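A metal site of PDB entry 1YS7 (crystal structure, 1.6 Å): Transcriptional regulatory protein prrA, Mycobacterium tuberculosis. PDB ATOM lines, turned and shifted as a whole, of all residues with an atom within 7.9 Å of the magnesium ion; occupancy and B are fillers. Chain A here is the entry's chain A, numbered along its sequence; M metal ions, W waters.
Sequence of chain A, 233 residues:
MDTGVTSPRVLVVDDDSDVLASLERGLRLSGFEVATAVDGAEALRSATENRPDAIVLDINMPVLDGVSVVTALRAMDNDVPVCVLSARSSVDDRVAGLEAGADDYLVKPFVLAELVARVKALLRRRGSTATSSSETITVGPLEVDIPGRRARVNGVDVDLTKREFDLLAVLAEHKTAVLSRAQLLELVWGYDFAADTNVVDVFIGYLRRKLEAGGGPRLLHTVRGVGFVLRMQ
The side-chain carboxylate (OD1) of Asp 15 is bound to the magnesium ion, 2.0 Å away.
The magnesium ion is bound by the side-chain carboxylate (OD2) of Asp 58 (2.0 Å).
Water W3 is bound to the magnesium ion, 2.0 Å away.
Water W2 binds the magnesium ion, 2.1 Å away.
The magnesium ion is bound by water W1 (2.1 Å).
The magnesium ion is bound by O of Asn 60, at 2.1 Å.
Water W3 lies within hydrogen-bond range of the side-chain carboxylate (OD1) of Asp 14 (2.7 Å) and the side-chain amino group (NZ) of Lys 108 (3.3 Å).
Merely in contact with the magnesium ion: Asp 14 (3.96 Å).
Of the 13 residues printed, 4 come within 4 Å of the magnesium ion.
The nearest printed residue that does not touch the magnesium ion is Met 61 (4.2 Å).
N of Asp 58 sits at hydrogen-bond distance from O of Val 13 (2.9 Å).
The side-chain carboxylate (OD2) of Asp 14 is in salt-bridge range of the side-chain amino group (NZ) of Lys 108 (2.6 Å).
The side-chain amino group (NZ) of Lys 108 is in salt-bridge range of the side-chain carboxylate (OD1) of Asp 58.
The side-chain carboxylate (OD1) of Asp 14 is in hydrogen-bond range of the backbone NH (N) of Asp 16 (2.8 Å).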
ATOM      1  N   VAL A  13      14.233 -25.205  11.628  1.00  0.00           N
ATOM      2  CA  VAL A  13      13.861 -24.638  10.332  1.00  0.00           C
ATOM      3  C   VAL A  13      12.465 -25.075   9.950  1.00  0.00           C
ATOM      4  O   VAL A  13      12.198 -26.263   9.802  1.00  0.00           O
ATOM      5  CB  VAL A  13      14.833 -25.079   9.218  1.00  0.00           C
ATOM      6  CG1 VAL A  13      14.590 -24.333   7.926  1.00  0.00           C
ATOM      7  CG2 VAL A  13      16.323 -24.945   9.624  1.00  0.00           C
ATOM      8  N   ASP A  14      11.525 -24.116   9.814  1.00  0.00           N
ATOM      9  CA  ASP A  14      10.161 -24.480   9.413  1.00  0.00           C
ATOM     10  C   ASP A  14       9.512 -23.198   8.879  1.00  0.00           C
ATOM     11  O   ASP A  14       9.741 -22.089   9.466  1.00  0.00           O
ATOM     12  CB  ASP A  14       9.383 -25.008  10.610  1.00  0.00           C
ATOM     13  CG  ASP A  14       8.172 -25.813  10.205  1.00  0.00           C
ATOM     14  OD1 ASP A  14       7.304 -25.269   9.503  1.00  0.00           O
ATOM     15  OD2 ASP A  14       8.136 -27.017  10.529  1.00  0.00           O
ATOM     16  N   ASP A  15       8.742 -23.334   7.796  1.00  0.00           N
ATOM     17  CA  ASP A  15       8.134 -22.148   7.171  1.00  0.00           C
ATOM     18  C   ASP A  15       6.815 -21.841   7.827  1.00  0.00           C
ATOM     19  O   ASP A  15       6.177 -20.825   7.508  1.00  0.00           O
ATOM     20  CB  ASP A  15       7.893 -22.341   5.671  1.00  0.00           C
ATOM     21  CG  ASP A  15       7.065 -23.563   5.371  1.00  0.00           C
ATOM     22  OD1 ASP A  15       7.278 -24.670   5.941  1.00  0.00           O
ATOM     23  OD2 ASP A  15       6.148 -23.458   4.533  1.00  0.00           O
ATOM     24  N   ASP A  16       6.391 -22.706   8.738  1.00  0.00           N
ATOM     25  CA  ASP A  16       5.178 -22.425   9.487  1.00  0.00           C
ATOM     26  C   ASP A  16       5.585 -21.690  10.740  1.00  0.00           C
ATOM     27  O   ASP A  16       6.137 -22.278  11.675  1.00  0.00           O
ATOM     28  CB  ASP A  16       4.496 -23.736   9.832  1.00  0.00           C
ATOM     29  CG  ASP A  16       3.175 -23.540  10.578  1.00  0.00           C
ATOM     30  OD1 ASP A  16       2.183 -24.232  10.251  1.00  0.00           O
ATOM     31  OD2 ASP A  16       3.121 -22.740  11.533  1.00  0.00           O
ATOM     32  N   VAL A  19       4.617 -23.227  14.183  1.00  0.00           N
ATOM     33  CA  VAL A  19       5.364 -24.412  14.528  1.00  0.00           C
ATOM     34  C   VAL A  19       6.779 -24.010  14.917  1.00  0.00           C
ATOM     35  O   VAL A  19       7.283 -24.499  15.923  1.00  0.00           O
ATOM     36  CB  VAL A  19       5.439 -25.390  13.365  1.00  0.00           C
ATOM     37  CG1 VAL A  19       6.483 -26.475  13.675  1.00  0.00           C
ATOM     38  CG2 VAL A  19       4.115 -26.015  13.169  1.00  0.00           C
ATOM     39  N   VAL A  38      13.331 -19.571   8.571  1.00  0.00           N
ATOM     40  CA  VAL A  38      11.964 -19.739   8.042  1.00  0.00           C
ATOM     41  C   VAL A  38      11.911 -20.464   6.724  1.00  0.00           C
ATOM     42  O   VAL A  38      10.842 -20.803   6.248  1.00  0.00           O
ATOM     43  CB  VAL A  38      11.207 -18.372   7.897  1.00  0.00           C
ATOM     44  CG1 VAL A  38      11.229 -17.658   9.254  1.00  0.00           C
ATOM     45  CG2 VAL A  38      11.908 -17.489   6.835  1.00  0.00           C
ATOM     46  N   ASP A  58      12.465 -28.861   8.470  1.00  0.00           N
ATOM     47  CA  ASP A  58      11.199 -29.170   7.796  1.00  0.00           C
ATOM     48  C   ASP A  58      11.473 -29.452   6.336  1.00  0.00           C
ATOM     49  O   ASP A  58      12.384 -28.908   5.766  1.00  0.00           O
ATOM     50  CB  ASP A  58      10.280 -27.968   7.969  1.00  0.00           C
ATOM     51  CG  ASP A  58       8.901 -28.172   7.357  1.00  0.00           C
ATOM     52  OD1 ASP A  58       8.305 -29.254   7.523  1.00  0.00           O
ATOM     53  OD2 ASP A  58       8.404 -27.221   6.688  1.00  0.00           O
ATOM     54  N   ILE A  59      10.630 -30.238   5.681  1.00  0.00           N
ATOM     55  CA  ILE A  59      10.881 -30.558   4.280  1.00  0.00           C
ATOM     56  C   ILE A  59      10.204 -29.548   3.340  1.00  0.00           C
ATOM     57  O   ILE A  59      10.848 -28.945   2.506  1.00  0.00           O
ATOM     58  CB  ILE A  59      10.472 -32.030   3.949  1.00  0.00           C
ATOM     59  CG1 ILE A  59      11.406 -33.011   4.718  1.00  0.00           C
ATOM     60  CG2 ILE A  59      10.552 -32.298   2.397  1.00  0.00           C
ATOM     61  CD1 ILE A  59      12.890 -32.848   4.343  1.00  0.00           C
ATOM     62  N   ASN A  60       8.877 -29.432   3.437  1.00  0.00           N
ATOM     63  CA  ASN A  60       8.152 -28.570   2.506  1.00  0.00           C
ATOM     64  C   ASN A  60       8.233 -27.099   2.928  1.00  0.00           C
ATOM     65  O   ASN A  60       7.635 -26.726   3.928  1.00  0.00           O
ATOM     66  CB  ASN A  60       6.682 -29.015   2.414  1.00  0.00           C
ATOM     67  CG  ASN A  60       6.517 -30.432   1.833  1.00  0.00           C
ATOM     68  OD1 ASN A  60       5.522 -31.103   2.102  1.00  0.00           O
ATOM     69  ND2 ASN A  60       7.494 -30.895   1.047  1.00  0.00           N
ATOM     70  N   MET A  61       9.033 -26.300   2.216  1.00  0.00           N
ATOM     71  CA  MET A  61       9.216 -24.878   2.455  1.00  0.00           C
ATOM     72  C   MET A  61       9.411 -24.176   1.121  1.00  0.00           C
ATOM     73  O   MET A  61       9.932 -24.775   0.128  1.00  0.00           O
ATOM     74  CB  MET A  61      10.508 -24.595   3.298  1.00  0.00           C
ATOM     75  CG  MET A  61      10.575 -25.333   4.583  1.00  0.00           C
ATOM     76  SD  MET A  61      12.012 -24.975   5.582  1.00  0.00           S
ATOM     77  CE  MET A  61      13.315 -25.698   4.622  1.00  0.00           C
ATOM     78  N   PRO A  62       9.069 -22.861   1.086  1.00  0.00           N
ATOM     79  CA  PRO A  62       9.368 -22.070  -0.088  1.00  0.00           C
ATOM     80  C   PRO A  62      10.844 -21.728  -0.164  1.00  0.00           C
ATOM     81  O   PRO A  62      11.560 -21.964   0.809  1.00  0.00           O
ATOM     82  CB  PRO A  62       8.540 -20.801   0.153  1.00  0.00           C
ATOM     83  CG  PRO A  62       8.518 -20.641   1.618  1.00  0.00           C
ATOM     84  CD  PRO A  62       8.386 -22.077   2.129  1.00  0.00           C
ATOM     85  N   LEU A  85      11.754 -33.185   9.488  1.00  0.00           N
ATOM     86  CA  LEU A  85      10.325 -33.304   9.836  1.00  0.00           C
ATOM     87  C   LEU A  85       9.636 -33.516   8.515  1.00  0.00           C
ATOM     88  O   LEU A  85       9.630 -32.635   7.667  1.00  0.00           O
ATOM     89  CB  LEU A  85       9.830 -32.006  10.474  1.00  0.00           C
ATOM     90  CG  LEU A  85      10.689 -31.465  11.606  1.00  0.00           C
ATOM     91  CD1 LEU A  85      10.117 -30.147  12.165  1.00  0.00           C
ATOM     92  CD2 LEU A  85      10.852 -32.501  12.710  1.00  0.00           C
ATOM     93  N   LYS A 108       5.275 -35.104  11.540  1.00  0.00           N
ATOM     94  CA  LYS A 108       4.268 -34.247  12.187  1.00  0.00           C
ATOM     95  C   LYS A 108       2.877 -34.872  12.039  1.00  0.00           C
ATOM     96  O   LYS A 108       2.564 -35.447  10.978  1.00  0.00           O
ATOM     97  CB  LYS A 108       4.214 -32.882  11.517  1.00  0.00           C
ATOM     98  CG  LYS A 108       5.401 -32.006  11.715  1.00  0.00           C
ATOM     99  CD  LYS A 108       5.256 -30.782  10.816  1.00  0.00           C
ATOM    100  CE  LYS A 108       6.459 -29.864  10.933  1.00  0.00           C
ATOM    101  NZ  LYS A 108       6.464 -28.832   9.830  1.00  0.00           N
HETATM  102 MG    MG M   1       6.702 -26.555   5.808  1.00  0.00          MG
HETATM  103  O   HOH W   1       4.943 -25.893   4.862  1.00  0.00           O
HETATM  104  O   HOH W   2       6.035 -28.537   5.665  1.00  0.00           O
HETATM  105  O   HOH W   3       5.753 -26.490   7.601  1.00  0.00           O
